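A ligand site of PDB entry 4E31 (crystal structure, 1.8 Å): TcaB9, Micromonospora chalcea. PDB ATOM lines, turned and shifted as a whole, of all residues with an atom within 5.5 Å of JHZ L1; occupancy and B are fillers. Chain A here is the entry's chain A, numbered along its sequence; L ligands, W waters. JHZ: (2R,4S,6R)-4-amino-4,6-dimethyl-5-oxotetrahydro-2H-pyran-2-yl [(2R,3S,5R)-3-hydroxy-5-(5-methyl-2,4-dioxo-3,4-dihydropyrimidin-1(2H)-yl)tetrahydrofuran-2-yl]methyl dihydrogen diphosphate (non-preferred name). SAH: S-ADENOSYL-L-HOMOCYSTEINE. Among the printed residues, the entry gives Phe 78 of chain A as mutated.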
ATOM      1  N   ASP A  35      18.115 -26.806  -5.327  1.00  0.00           N
ATOM      2  CA  ASP A  35      18.927 -26.006  -6.212  1.00  0.00           C
ATOM      3  C   ASP A  35      18.112 -25.451  -7.371  1.00  0.00           C
ATOM      4  O   ASP A  35      18.723 -25.044  -8.343  1.00  0.00           O
ATOM      5  CB  ASP A  35      20.181 -26.774  -6.648  1.00  0.00           C
ATOM      6  CG  ASP A  35      21.416 -26.375  -5.836  1.00  0.00           C
ATOM      7  OD1 ASP A  35      21.614 -25.178  -5.561  1.00  0.00           O
ATOM      8  OD2 ASP A  35      22.195 -27.289  -5.441  1.00  0.00           O
ATOM      9  N   PHE A  78      21.818 -26.876 -13.363  1.00  0.00           N
ATOM     10  CA  PHE A  78      22.307 -26.985 -12.010  1.00  0.00           C
ATOM     11  C   PHE A  78      23.215 -25.749 -11.811  1.00  0.00           C
ATOM     12  O   PHE A  78      24.114 -25.462 -12.620  1.00  0.00           O
ATOM     13  CB  PHE A  78      23.086 -28.297 -11.884  1.00  0.00           C
ATOM     14  CG  PHE A  78      23.878 -28.359 -10.601  1.00  0.00           C
ATOM     15  CD1 PHE A  78      23.268 -28.739  -9.415  1.00  0.00           C
ATOM     16  CD2 PHE A  78      25.237 -28.092 -10.604  1.00  0.00           C
ATOM     17  CE1 PHE A  78      23.990 -28.837  -8.204  1.00  0.00           C
ATOM     18  CE2 PHE A  78      25.989 -28.201  -9.414  1.00  0.00           C
ATOM     19  CZ  PHE A  78      25.365 -28.563  -8.218  1.00  0.00           C
ATOM     20  N   TYR A  80      25.290 -24.460  -9.194  1.00  0.00           N
ATOM     21  CA  TYR A  80      26.331 -24.133  -8.202  1.00  0.00           C
ATOM     22  C   TYR A  80      27.685 -23.950  -8.893  1.00  0.00           C
ATOM     23  O   TYR A  80      28.105 -24.862  -9.627  1.00  0.00           O
ATOM     24  CB  TYR A  80      26.502 -25.279  -7.199  1.00  0.00           C
ATOM     25  CG  TYR A  80      27.516 -24.972  -6.126  1.00  0.00           C
ATOM     26  CD1 TYR A  80      27.309 -23.987  -5.173  1.00  0.00           C
ATOM     27  CD2 TYR A  80      28.734 -25.686  -6.093  1.00  0.00           C
ATOM     28  CE1 TYR A  80      28.272 -23.702  -4.211  1.00  0.00           C
ATOM     29  CE2 TYR A  80      29.695 -25.418  -5.146  1.00  0.00           C
ATOM     30  CZ  TYR A  80      29.446 -24.427  -4.214  1.00  0.00           C
ATOM     31  OH  TYR A  80      30.374 -24.229  -3.228  1.00  0.00           O
ATOM     32  N   GLY A  84      33.127 -19.736  -6.981  1.00  0.00           N
ATOM     33  CA  GLY A  84      32.646 -18.460  -6.463  1.00  0.00           C
ATOM     34  C   GLY A  84      33.195 -18.259  -5.062  1.00  0.00           C
ATOM     35  O   GLY A  84      32.864 -17.270  -4.430  1.00  0.00           O
ATOM     36  N   SER A  85      34.043 -19.136  -4.536  1.00  0.00           N
ATOM     37  CA  SER A  85      34.649 -18.897  -3.216  1.00  0.00           C
ATOM     38  C   SER A  85      36.178 -18.896  -3.316  1.00  0.00           C
ATOM     39  O   SER A  85      36.749 -19.838  -3.860  1.00  0.00           O
ATOM     40  CB  SER A  85      34.247 -20.021  -2.275  1.00  0.00           C
ATOM     41  OG  SER A  85      35.071 -19.999  -1.120  1.00  0.00           O
ATOM     42  N   ASN A 179      32.652 -33.218  -2.372  1.00  0.00           N
ATOM     43  CA  ASN A 179      31.254 -32.775  -2.335  1.00  0.00           C
ATOM     44  C   ASN A 179      30.437 -33.405  -3.464  1.00  0.00           C
ATOM     45  O   ASN A 179      29.613 -32.708  -4.055  1.00  0.00           O
ATOM     46  CB  ASN A 179      31.153 -31.248  -2.371  1.00  0.00           C
ATOM     47  CG  ASN A 179      32.052 -30.677  -1.295  1.00  0.00           C
ATOM     48  OD1 ASN A 179      31.735 -30.997  -0.147  1.00  0.00           O
ATOM     49  ND2 ASN A 179      33.155 -29.993  -1.601  1.00  0.00           N
ATOM     50  N   HIS A 183      26.549 -37.409  -2.630  1.00  0.00           N
ATOM     51  CA  HIS A 183      25.370 -36.956  -3.401  1.00  0.00           C
ATOM     52  C   HIS A 183      24.809 -38.122  -4.229  1.00  0.00           C
ATOM     53  O   HIS A 183      23.760 -37.979  -4.877  1.00  0.00           O
ATOM     54  CB  HIS A 183      25.758 -35.917  -4.460  1.00  0.00           C
ATOM     55  CG  HIS A 183      26.198 -34.608  -3.878  1.00  0.00           C
ATOM     56  ND1 HIS A 183      26.998 -34.489  -2.750  1.00  0.00           N
ATOM     57  CD2 HIS A 183      25.848 -33.353  -4.222  1.00  0.00           C
ATOM     58  CE1 HIS A 183      27.138 -33.206  -2.468  1.00  0.00           C
ATOM     59  NE2 HIS A 183      26.477 -32.496  -3.364  1.00  0.00           N
ATOM     60  N   TYR A 224      19.698 -32.203   2.872  1.00  0.00           N
ATOM     61  CA  TYR A 224      18.781 -31.765   1.828  1.00  0.00           C
ATOM     62  C   TYR A 224      18.954 -32.764   0.657  1.00  0.00           C
ATOM     63  O   TYR A 224      19.772 -33.695   0.732  1.00  0.00           O
ATOM     64  CB  TYR A 224      19.094 -30.301   1.488  1.00  0.00           C
ATOM     65  CG  TYR A 224      20.468 -30.005   0.923  1.00  0.00           C
ATOM     66  CD1 TYR A 224      20.719 -30.016  -0.451  1.00  0.00           C
ATOM     67  CD2 TYR A 224      21.527 -29.687   1.780  1.00  0.00           C
ATOM     68  CE1 TYR A 224      21.964 -29.670  -0.984  1.00  0.00           C
ATOM     69  CE2 TYR A 224      22.788 -29.379   1.247  1.00  0.00           C
ATOM     70  CZ  TYR A 224      22.997 -29.380  -0.126  1.00  0.00           C
ATOM     71  OH  TYR A 224      24.247 -29.083  -0.625  1.00  0.00           O
ATOM     72  N   GLU A 226      20.391 -33.204  -2.253  1.00  0.00           N
ATOM     73  CA  GLU A 226      21.653 -33.595  -2.869  1.00  0.00           C
ATOM     74  C   GLU A 226      22.604 -34.303  -1.896  1.00  0.00           C
ATOM     75  O   GLU A 226      23.634 -34.830  -2.355  1.00  0.00           O
ATOM     76  CB  GLU A 226      22.330 -32.330  -3.411  1.00  0.00           C
ATOM     77  CG  GLU A 226      21.566 -31.747  -4.630  1.00  0.00           C
ATOM     78  CD  GLU A 226      22.125 -30.415  -5.095  1.00  0.00           C
ATOM     79  OE1 GLU A 226      23.334 -30.136  -4.871  1.00  0.00           O
ATOM     80  OE2 GLU A 226      21.342 -29.647  -5.691  1.00  0.00           O
ATOM     81  N   HIS A 227      22.305 -34.304  -0.602  1.00  0.00           N
ATOM     82  CA  HIS A 227      23.216 -34.903   0.381  1.00  0.00           C
ATOM     83  C   HIS A 227      22.573 -36.223   0.804  1.00  0.00           C
ATOM     84  O   HIS A 227      21.892 -36.220   1.830  1.00  0.00           O
ATOM     85  CB  HIS A 227      23.414 -33.956   1.597  1.00  0.00           C
ATOM     86  CG  HIS A 227      24.429 -32.887   1.281  1.00  0.00           C
ATOM     87  ND1 HIS A 227      24.852 -31.951   2.189  1.00  0.00           N
ATOM     88  CD2 HIS A 227      25.079 -32.606   0.128  1.00  0.00           C
ATOM     89  CE1 HIS A 227      25.718 -31.122   1.639  1.00  0.00           C
ATOM     90  NE2 HIS A 227      25.902 -31.527   0.382  1.00  0.00           N
ATOM     91  N   HIS A 256      33.126 -26.140   4.365  1.00  0.00           N
ATOM     92  CA  HIS A 256      31.742 -26.584   4.192  1.00  0.00           C
ATOM     93  C   HIS A 256      31.164 -27.030   5.517  1.00  0.00           C
ATOM     94  O   HIS A 256      30.366 -27.979   5.546  1.00  0.00           O
ATOM     95  CB  HIS A 256      31.596 -27.668   3.118  1.00  0.00           C
ATOM     96  CG  HIS A 256      31.706 -27.111   1.737  1.00  0.00           C
ATOM     97  ND1 HIS A 256      30.854 -26.130   1.256  1.00  0.00           N
ATOM     98  CD2 HIS A 256      32.585 -27.382   0.735  1.00  0.00           C
ATOM     99  CE1 HIS A 256      31.220 -25.811   0.026  1.00  0.00           C
ATOM    100  NE2 HIS A 256      32.254 -26.561  -0.323  1.00  0.00           N
ATOM    101  N   TYR A 325      21.827 -13.959   3.656  1.00  0.00           N
ATOM    102  CA  TYR A 325      23.016 -13.805   2.811  1.00  0.00           C
ATOM    103  C   TYR A 325      23.509 -15.196   2.429  1.00  0.00           C
ATOM    104  O   TYR A 325      23.841 -16.016   3.295  1.00  0.00           O
ATOM    105  CB  TYR A 325      24.060 -13.027   3.588  1.00  0.00           C
ATOM    106  CG  TYR A 325      25.137 -12.422   2.722  1.00  0.00           C
ATOM    107  CD1 TYR A 325      26.027 -13.236   2.012  1.00  0.00           C
ATOM    108  CD2 TYR A 325      25.323 -11.042   2.695  1.00  0.00           C
ATOM    109  CE1 TYR A 325      27.055 -12.642   1.220  1.00  0.00           C
ATOM    110  CE2 TYR A 325      26.312 -10.457   1.914  1.00  0.00           C
ATOM    111  CZ  TYR A 325      27.168 -11.262   1.178  1.00  0.00           C
ATOM    112  OH  TYR A 325      28.163 -10.664   0.435  1.00  0.00           O
ATOM    113  N   GLY A 326      23.515 -15.400   1.113  1.00  0.00           N
ATOM    114  CA  GLY A 326      23.964 -16.679   0.563  1.00  0.00           C
ATOM    115  C   GLY A 326      22.740 -17.475   0.161  1.00  0.00           C
ATOM    116  O   GLY A 326      22.043 -17.988   1.008  1.00  0.00           O
ATOM    117  N   ALA A 327      22.484 -17.619  -1.143  1.00  0.00           N
ATOM    118  CA  ALA A 327      21.335 -18.456  -1.557  1.00  0.00           C
ATOM    119  C   ALA A 327      21.803 -19.919  -1.677  1.00  0.00           C
ATOM    120  O   ALA A 327      21.828 -20.521  -2.765  1.00  0.00           O
ATOM    121  CB  ALA A 327      20.787 -17.973  -2.940  1.00  0.00           C
ATOM    122  N   THR A 328      22.215 -20.472  -0.547  1.00  0.00           N
ATOM    123  CA  THR A 328      22.726 -21.846  -0.502  1.00  0.00           C
ATOM    124  C   THR A 328      21.634 -22.875  -0.821  1.00  0.00           C
ATOM    125  O   THR A 328      20.467 -22.656  -0.508  1.00  0.00           O
ATOM    126  CB  THR A 328      23.194 -22.176   0.923  1.00  0.00           C
ATOM    127  OG1 THR A 328      22.123 -21.953   1.852  1.00  0.00           O
ATOM    128  CG2 THR A 328      24.370 -21.200   1.256  1.00  0.00           C
ATOM    129  N   ALA A 329      22.055 -24.013  -1.358  1.00  0.00           N
ATOM    130  CA  ALA A 329      21.205 -25.191  -1.408  1.00  0.00           C
ATOM    131  C   ALA A 329      20.779 -25.531   0.027  1.00  0.00           C
ATOM    132  O   ALA A 329      19.618 -25.846   0.280  1.00  0.00           O
ATOM    133  CB  ALA A 329      22.018 -26.347  -1.962  1.00  0.00           C
ATOM    134  N   LYS A 330      21.686 -25.480   0.999  1.00  0.00           N
ATOM    135  CA  LYS A 330      21.363 -25.709   2.393  1.00  0.00           C
ATOM    136  C   LYS A 330      20.169 -24.926   2.891  1.00  0.00           C
ATOM    137  O   LYS A 330      19.394 -25.436   3.698  1.00  0.00           O
ATOM    138  CB  LYS A 330      22.547 -25.340   3.302  1.00  0.00           C
ATOM    139  CG  LYS A 330      23.777 -26.229   3.020  1.00  0.00           C
ATOM    140  CD  LYS A 330      24.930 -25.981   4.051  1.00  0.00           C
ATOM    141  CE  LYS A 330      25.480 -24.543   4.053  1.00  0.00           C
ATOM    142  NZ  LYS A 330      26.365 -24.421   2.841  1.00  0.00           N
ATOM    143  N   TYR A 349      20.813 -12.281  -0.569  1.00  0.00           N
ATOM    144  CA  TYR A 349      21.857 -11.748  -1.456  1.00  0.00           C
ATOM    145  C   TYR A 349      22.849 -12.857  -1.860  1.00  0.00           C
ATOM    146  O   TYR A 349      23.303 -13.665  -1.053  1.00  0.00           O
ATOM    147  CB  TYR A 349      22.582 -10.575  -0.762  1.00  0.00           C
ATOM    148  CG  TYR A 349      21.590  -9.457  -0.567  1.00  0.00           C
ATOM    149  CD1 TYR A 349      21.248  -8.619  -1.629  1.00  0.00           C
ATOM    150  CD2 TYR A 349      20.881  -9.356   0.638  1.00  0.00           C
ATOM    151  CE1 TYR A 349      20.262  -7.630  -1.492  1.00  0.00           C
ATOM    152  CE2 TYR A 349      19.915  -8.401   0.783  1.00  0.00           C
ATOM    153  CZ  TYR A 349      19.637  -7.545  -0.268  1.00  0.00           C
ATOM    154  OH  TYR A 349      18.631  -6.638  -0.021  1.00  0.00           O
ATOM    155  N   ASP A 350      23.226 -12.888  -3.135  1.00  0.00           N
ATOM    156  CA  ASP A 350      24.057 -13.990  -3.604  1.00  0.00           C
ATOM    157  C   ASP A 350      24.871 -13.636  -4.866  1.00  0.00           C
ATOM    158  O   ASP A 350      24.404 -12.857  -5.712  1.00  0.00           O
ATOM    159  CB  ASP A 350      23.133 -15.157  -3.975  1.00  0.00           C
ATOM    160  CG  ASP A 350      23.915 -16.455  -4.145  1.00  0.00           C
ATOM    161  OD1 ASP A 350      24.108 -17.244  -3.199  1.00  0.00           O
ATOM    162  OD2 ASP A 350      24.316 -16.705  -5.298  1.00  0.00           O
ATOM    163  N   THR A 351      26.062 -14.215  -4.997  1.00  0.00           N
ATOM    164  CA  THR A 351      26.912 -13.781  -6.111  1.00  0.00           C
ATOM    165  C   THR A 351      26.723 -14.590  -7.375  1.00  0.00           C
ATOM    166  O   THR A 351      27.425 -14.344  -8.354  1.00  0.00           O
ATOM    167  CB  THR A 351      28.403 -13.822  -5.693  1.00  0.00           C
ATOM    168  OG1 THR A 351      28.663 -15.097  -5.109  1.00  0.00           O
ATOM    169  CG2 THR A 351      28.679 -12.756  -4.668  1.00  0.00           C
ATOM    170  N   THR A 352      25.813 -15.566  -7.380  1.00  0.00           N
ATOM    171  CA  THR A 352      25.707 -16.454  -8.532  1.00  0.00           C
ATOM    172  C   THR A 352      24.721 -15.843  -9.526  1.00  0.00           C
ATOM    173  O   THR A 352      23.538 -15.705  -9.213  1.00  0.00           O
ATOM    174  CB  THR A 352      25.158 -17.837  -8.107  1.00  0.00           C
ATOM    175  OG1 THR A 352      25.834 -18.331  -6.942  1.00  0.00           O
ATOM    176  CG2 THR A 352      25.389 -18.852  -9.199  1.00  0.00           C
ATOM    177  N   LYS A 355      21.338 -17.462 -10.043  1.00  0.00           N
ATOM    178  CA  LYS A 355      20.399 -17.470  -8.912  1.00  0.00           C
ATOM    179  C   LYS A 355      19.732 -16.111  -8.679  1.00  0.00           C
ATOM    180  O   LYS A 355      18.686 -16.064  -8.044  1.00  0.00           O
ATOM    181  CB  LYS A 355      21.046 -17.895  -7.589  1.00  0.00           C
ATOM    182  CG  LYS A 355      21.673 -19.308  -7.550  1.00  0.00           C
ATOM    183  CD  LYS A 355      22.325 -19.589  -6.182  1.00  0.00           C
ATOM    184  CE  LYS A 355      23.107 -20.919  -6.239  1.00  0.00           C
ATOM    185  NZ  LYS A 355      23.369 -21.427  -4.840  1.00  0.00           N
ATOM    186  N   ALA A 370      24.668  -9.731  -4.655  1.00  0.00           N
ATOM    187  CA  ALA A 370      25.281  -9.297  -3.387  1.00  0.00           C
ATOM    188  C   ALA A 370      25.729  -7.863  -3.543  1.00  0.00           C
ATOM    189  O   ALA A 370      25.898  -7.124  -2.571  1.00  0.00           O
ATOM    190  CB  ALA A 370      26.519 -10.163  -3.096  1.00  0.00           C
ATOM    191  N   ALA A 385      25.074 -18.684   4.226  1.00  0.00           N
ATOM    192  CA  ALA A 385      26.412 -19.141   3.838  1.00  0.00           C
ATOM    193  C   ALA A 385      27.386 -19.107   5.017  1.00  0.00           C
ATOM    194  O   ALA A 385      28.494 -18.573   4.966  1.00  0.00           O
ATOM    195  CB  ALA A 385      26.924 -18.361   2.578  1.00  0.00           C
ATOM    196  N   ASN A 387      29.127 -21.365   6.339  1.00  0.00           N
ATOM    197  CA  ASN A 387      30.382 -22.081   6.116  1.00  0.00           C
ATOM    198  C   ASN A 387      31.454 -21.178   5.463  1.00  0.00           C
ATOM    199  O   ASN A 387      32.641 -21.539   5.453  1.00  0.00           O
ATOM    200  CB  ASN A 387      30.144 -23.347   5.305  1.00  0.00           C
ATOM    201  CG  ASN A 387      29.295 -23.072   4.061  1.00  0.00           C
ATOM    202  OD1 ASN A 387      28.176 -22.580   4.145  1.00  0.00           O
ATOM    203  ND2 ASN A 387      29.867 -23.339   2.903  1.00  0.00           N
ATOM    204  N   HIS A 388      30.967 -20.042   4.963  1.00  0.00           N
ATOM    205  CA  HIS A 388      31.797 -19.006   4.324  1.00  0.00           C
ATOM    206  C   HIS A 388      31.909 -17.748   5.170  1.00  0.00           C
ATOM    207  O   HIS A 388      32.225 -16.705   4.607  1.00  0.00           O
ATOM    208  CB  HIS A 388      31.246 -18.633   2.938  1.00  0.00           C
ATOM    209  CG  HIS A 388      31.267 -19.752   1.941  1.00  0.00           C
ATOM    210  ND1 HIS A 388      32.448 -20.229   1.415  1.00  0.00           N
ATOM    211  CD2 HIS A 388      30.268 -20.421   1.306  1.00  0.00           C
ATOM    212  CE1 HIS A 388      32.179 -21.184   0.535  1.00  0.00           C
ATOM    213  NE2 HIS A 388      30.864 -21.326   0.456  1.00  0.00           N
ATOM    214  N   GLU A 391      35.167 -15.510   4.904  1.00  0.00           N
ATOM    215  CA  GLU A 391      35.334 -14.913   3.597  1.00  0.00           C
ATOM    216  C   GLU A 391      34.287 -13.810   3.369  1.00  0.00           C
ATOM    217  O   GLU A 391      34.573 -12.753   2.788  1.00  0.00           O
ATOM    218  CB  GLU A 391      35.236 -15.991   2.524  1.00  0.00           C
ATOM    219  CG  GLU A 391      35.431 -15.460   1.119  1.00  0.00           C
ATOM    220  CD  GLU A 391      35.364 -16.559   0.078  1.00  0.00           C
ATOM    221  OE1 GLU A 391      35.092 -16.190  -1.079  1.00  0.00           O
ATOM    222  OE2 GLU A 391      35.588 -17.756   0.388  1.00  0.00           O
ATOM    223  N   ILE A 392      33.047 -14.084   3.743  1.00  0.00           N
ATOM    224  CA  ILE A 392      31.947 -13.163   3.485  1.00  0.00           C
ATOM    225  C   ILE A 392      32.082 -11.938   4.384  1.00  0.00           C
ATOM    226  O   ILE A 392      31.938 -10.782   3.953  1.00  0.00           O
ATOM    227  CB  ILE A 392      30.571 -13.836   3.675  1.00  0.00           C
ATOM    228  CG1 ILE A 392      30.270 -14.743   2.484  1.00  0.00           C
ATOM    229  CG2 ILE A 392      29.450 -12.780   3.788  1.00  0.00           C
ATOM    230  CD1 ILE A 392      29.004 -15.623   2.681  1.00  0.00           C
ATOM    231  N   LYS A 395      34.487  -9.318   3.327  1.00  0.00           N
ATOM    232  CA  LYS A 395      34.080  -8.521   2.157  1.00  0.00           C
ATOM    233  C   LYS A 395      32.982  -7.565   2.587  1.00  0.00           C
ATOM    234  O   LYS A 395      32.697  -6.612   1.862  1.00  0.00           O
ATOM    235  CB  LYS A 395      33.505  -9.445   1.082  1.00  0.00           C
ATOM    236  CG  LYS A 395      34.553 -10.313   0.401  1.00  0.00           C
ATOM    237  CD  LYS A 395      34.194 -10.700  -1.012  1.00  0.00           C
ATOM    238  CE  LYS A 395      32.938 -11.519  -0.933  1.00  0.00           C
ATOM    239  NZ  LYS A 395      32.800 -12.386  -2.119  1.00  0.00           N
HETATM  240  P   JHZ L   1      27.929 -22.967  -0.580  1.00  0.00           P
HETATM  241  C1  JHZ L   1      26.112 -26.418  -2.923  1.00  0.00           C
HETATM  242  O1  JHZ L   1      25.844 -26.265  -1.516  1.00  0.00           O
HETATM  243  C2  JHZ L   1      25.287 -27.583  -3.433  1.00  0.00           C
HETATM  244  P2  JHZ L   1      25.614 -24.770  -1.012  1.00  0.00           P
HETATM  245  C3  JHZ L   1      26.016 -28.933  -3.291  1.00  0.00           C
HETATM  246  N3  JHZ L   1      25.038 -29.994  -3.031  1.00  0.00           N
HETATM  247  C4  JHZ L   1      27.136 -28.900  -2.282  1.00  0.00           C
HETATM  248  O4  JHZ L   1      27.388 -29.749  -1.439  1.00  0.00           O
HETATM  249  C5  JHZ L   1      28.019 -27.692  -2.238  1.00  0.00           C
HETATM  250  O5  JHZ L   1      27.515 -26.657  -3.064  1.00  0.00           O
HETATM  251  C6  JHZ L   1      29.471 -27.961  -2.577  1.00  0.00           C
HETATM  252  C1X JHZ L   1      27.061 -17.445  -2.293  1.00  0.00           C
HETATM  253  N11 JHZ L   1      28.210 -16.640  -1.862  1.00  0.00           N
HETATM  254  O1P JHZ L   1      29.335 -22.959  -1.134  1.00  0.00           O
HETATM  255  C2X JHZ L   1      27.459 -18.333  -3.472  1.00  0.00           C
HETATM  256  C21 JHZ L   1      28.183 -15.293  -1.888  1.00  0.00           C
HETATM  257  O21 JHZ L   1      27.135 -14.727  -2.268  1.00  0.00           O
HETATM  258  O2P JHZ L   1      27.765 -22.858   0.936  1.00  0.00           O
HETATM  259  C3X JHZ L   1      26.632 -19.608  -3.340  1.00  0.00           C
HETATM  260  O3X JHZ L   1      25.340 -19.349  -3.891  1.00  0.00           O
HETATM  261  N31 JHZ L   1      29.250 -14.566  -1.480  1.00  0.00           N
HETATM  262  C3M JHZ L   1      26.747 -29.259  -4.596  1.00  0.00           C
HETATM  263  O3P JHZ L   1      25.144 -24.937   0.415  1.00  0.00           O
HETATM  264  C4X JHZ L   1      26.414 -19.602  -1.821  1.00  0.00           C
HETATM  265  O4X JHZ L   1      26.592 -18.312  -1.260  1.00  0.00           O
HETATM  266  C41 JHZ L   1      30.432 -15.111  -1.096  1.00  0.00           C
HETATM  267  O41 JHZ L   1      31.398 -14.396  -0.734  1.00  0.00           O
HETATM  268  O4P JHZ L   1      24.759 -23.936  -1.946  1.00  0.00           O
HETATM  269  C5X JHZ L   1      27.351 -20.469  -0.978  1.00  0.00           C
HETATM  270  O5X JHZ L   1      27.055 -21.822  -1.313  1.00  0.00           O
HETATM  271  C51 JHZ L   1      30.507 -16.595  -1.071  1.00  0.00           C
HETATM  272  C5A JHZ L   1      31.731 -17.373  -0.625  1.00  0.00           C
HETATM  273  C61 JHZ L   1      29.335 -17.265  -1.426  1.00  0.00           C
HETATM  274  OPP JHZ L   1      27.144 -24.269  -1.063  1.00  0.00           O
HETATM  275  N   SAH L   2      33.930 -30.802  -6.725  1.00  0.00           N
HETATM  276  CA  SAH L   2      33.200 -29.499  -6.664  1.00  0.00           C
HETATM  277  CB  SAH L   2      31.753 -29.585  -7.121  1.00  0.00           C
HETATM  278  CG  SAH L   2      30.726 -30.090  -6.111  1.00  0.00           C
HETATM  279  SD  SAH L   2      29.079 -29.891  -6.719  1.00  0.00           S
HETATM  280  C   SAH L   2      33.310 -28.858  -5.305  1.00  0.00           C
HETATM  281  O   SAH L   2      33.697 -29.556  -4.369  1.00  0.00           O
HETATM  282  OXT SAH L   2      32.991 -27.667  -5.103  1.00  0.00           O
HETATM  283  C5' SAH L   2      28.637 -31.590  -6.985  1.00  0.00           C
HETATM  284  C4' SAH L   2      28.852 -31.897  -8.460  1.00  0.00           C
HETATM  285  O4' SAH L   2      28.669 -33.297  -8.676  1.00  0.00           O
HETATM  286  C3' SAH L   2      27.831 -31.191  -9.365  1.00  0.00           C
HETATM  287  O3' SAH L   2      28.532 -30.384 -10.337  1.00  0.00           O
HETATM  288  C2' SAH L   2      27.145 -32.382 -10.031  1.00  0.00           C
HETATM  289  O2' SAH L   2      26.711 -32.252 -11.383  1.00  0.00           O
HETATM  290  C1' SAH L   2      28.208 -33.476 -10.005  1.00  0.00           C
HETATM  291  N9  SAH L   2      27.666 -34.873 -10.007  1.00  0.00           N
HETATM  292  C8  SAH L   2      26.539 -35.427  -9.493  1.00  0.00           C
HETATM  293  N7  SAH L   2      26.473 -36.779  -9.652  1.00  0.00           N
HETATM  294  C5  SAH L   2      27.633 -37.062 -10.313  1.00  0.00           C
HETATM  295  C6  SAH L   2      28.228 -38.328 -10.826  1.00  0.00           C
HETATM  296  N6  SAH L   2      27.586 -39.495 -10.707  1.00  0.00           N
HETATM  297  N1  SAH L   2      29.413 -38.220 -11.454  1.00  0.00           N
HETATM  298  C2  SAH L   2      30.037 -37.037 -11.609  1.00  0.00           C
HETATM  299  N3  SAH L   2      29.630 -35.841 -11.167  1.00  0.00           N
HETATM  300  C4  SAH L   2      28.421 -35.841 -10.522  1.00  0.00           C
HETATM  301  O   HOH W   1      31.215 -14.978  -4.345  1.00  0.00           O
HETATM  302  O   HOH W   2      29.065 -30.463   0.673  1.00  0.00           O
HETATM  303  O   HOH W   3      30.493 -20.164  -2.962  1.00  0.00           O
HETATM  304  O   HOH W   4      29.469 -11.746  -1.438  1.00  0.00           O
HETATM  305  O   HOH W   5      29.387 -20.084  -5.568  1.00  0.00           O
HETATM  306  O   HOH W   6      23.950 -24.052  -4.679  1.00  0.00           O
HETATM  307  O   HOH W   7      25.930 -27.688   1.077  1.00  0.00           O
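Asp 35 touches JHZ L1. Phe 78 touches JHZ L1. O of Gly 84 touches C5A of JHZ L1, at 3.97 Å. Asn 179 touches JHZ L1 (CB to C6, 3.7 Å). CE1 of His 256 touches O1P of JHZ L1, at 3.6 Å. Tyr 325 touches JHZ L1. Gly 326 touches JHZ L1 (CA to O4X, 3.6 Å). Ala 327 touches JHZ L1. CA of Thr 328 touches O4P of JHZ L1, 3.3 Å away. Ala 385 touches JHZ L1 (CB to O4X, 3.9 Å). Glu 391 touches JHZ L1. CG1 of Ile 392 touches O41 of JHZ L1, 3.4 Å away. The nearest printed residue that does not touch JHZ L1 is Ser 85 (4.01 Å).
Water W2 lies within hydrogen-bond range of an oxygen (O4) of JHZ L1 (2.8 Å), the side-chain amide oxygen (OD1) of Asn 179 (2.8 Å) and a ring nitrogen (NE2) of His 227 (3.3 Å). Water W4 lies within hydrogen-bond range of OH of Tyr 325, N31 of JHZ L1 and NZ of Lys 395. Water W6 lies within hydrogen-bond range of NZ of Lys 355 (2.7 Å), OD1 of Asp 35 (2.7 Å) and O4P of JHZ L1 (2.9 Å). Water W7 lies within hydrogen-bond range of OH of Tyr 224 and O3P of JHZ L1. Water W1 lies within hydrogen-bond range of the side-chain hydroxyl (OG1) of Thr 351 (2.7 Å), the backbone carbonyl oxygen (O) of Gly 84 (2.8 Å) and a nitrogen (N31) of JHZ L1 (3.5 Å).
The side-chain hydroxyl (OG1) of Thr 352 lies within hydrogen-bond range of the side-chain carboxylate (OD2) of Asp 350 (2.8 Å). The side-chain amide nitrogen (ND2) of Asn 387 lies within hydrogen-bond range of a ring nitrogen (NE2) of His 388, 3.3 Å away. N of Gly 326 is in hydrogen-bond range of O of Tyr 349. The backbone carbonyl oxygen (O) of Asp 350 sits at hydrogen-bond distance from the backbone NH (N) of Ala 370, 3.3 Å away. The side-chain amino group (NZ) of Lys 330 is in hydrogen-bond range of the side-chain amide oxygen (OD1) of Asn 387, 2.9 Å away. ND2 of Asn 387 lies within hydrogen-bond range of ND1 of His 256 (3.4 Å). The backbone carbonyl oxygen (O) of Ala 327 sits at hydrogen-bond distance from the side-chain amino group (NZ) of Lys 355 (2.7 Å). The side-chain carboxylate (OD2) of Asp 35 sits close to the side-chain carboxylate (OE2) of Glu 226 (2.5 Å).
OG1 of Thr 352 sits at hydrogen-bond distance from O3X of JHZ L1 (3.3 Å). An oxygen (O1P) of JHZ L1 is in hydrogen-bond range of a ring nitrogen (NE2) of His 388, at 2.7 Å. A nitrogen (N3) of JHZ L1 is in hydrogen-bond range of a ring nitrogen (NE2) of His 183, at 2.9 Å. ND2 of Asn 387 sits at hydrogen-bond distance from O2P of JHZ L1 (2.9 Å). A nitrogen (N3) of JHZ L1 lies within hydrogen-bond range of the side-chain hydroxyl (OH) of Tyr 224 (2.7 Å). An oxygen (O3X) of JHZ L1 lies within hydrogen-bond range of the side-chain carboxylate (OD1) of Asp 350, at 2.5 Å. An oxygen (O21) of JHZ L1 is in hydrogen-bond range of the backbone NH of Thr 351. The side-chain amino group (NZ) of Lys 330 lies within salt-bridge range of an oxygen (O3P) of JHZ L1. O4 of JHZ L1 lies within hydrogen-bond range of NE2 of His 227. An oxygen (O) of SAH L2 sits at hydrogen-bond distance from the side-chain amide nitrogen of Asn 179, 2.9 Å away. N of Ala 329 is in hydrogen-bond range of O4P of JHZ L1 (2.8 Å). The side-chain hydroxyl (OH) of Tyr 80 lies within hydrogen-bond range of an oxygen (O1P) of JHZ L1 (2.7 Å). O41 of JHZ L1 is in hydrogen-bond range of NZ of Lys 395, at 2.8 Å. An oxygen (O3X) of JHZ L1 is in hydrogen-bond range of the side-chain amino group (NZ) of Lys 355 (3.0 Å). A nitrogen (N3) of JHZ L1 is in salt-bridge range of the side-chain carboxylate (OE1) of Glu 226 (2.5 Å). The side-chain hydroxyl of Thr 351 sits at hydrogen-bond distance from an oxygen (O21) of JHZ L1 (3.2 Å).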
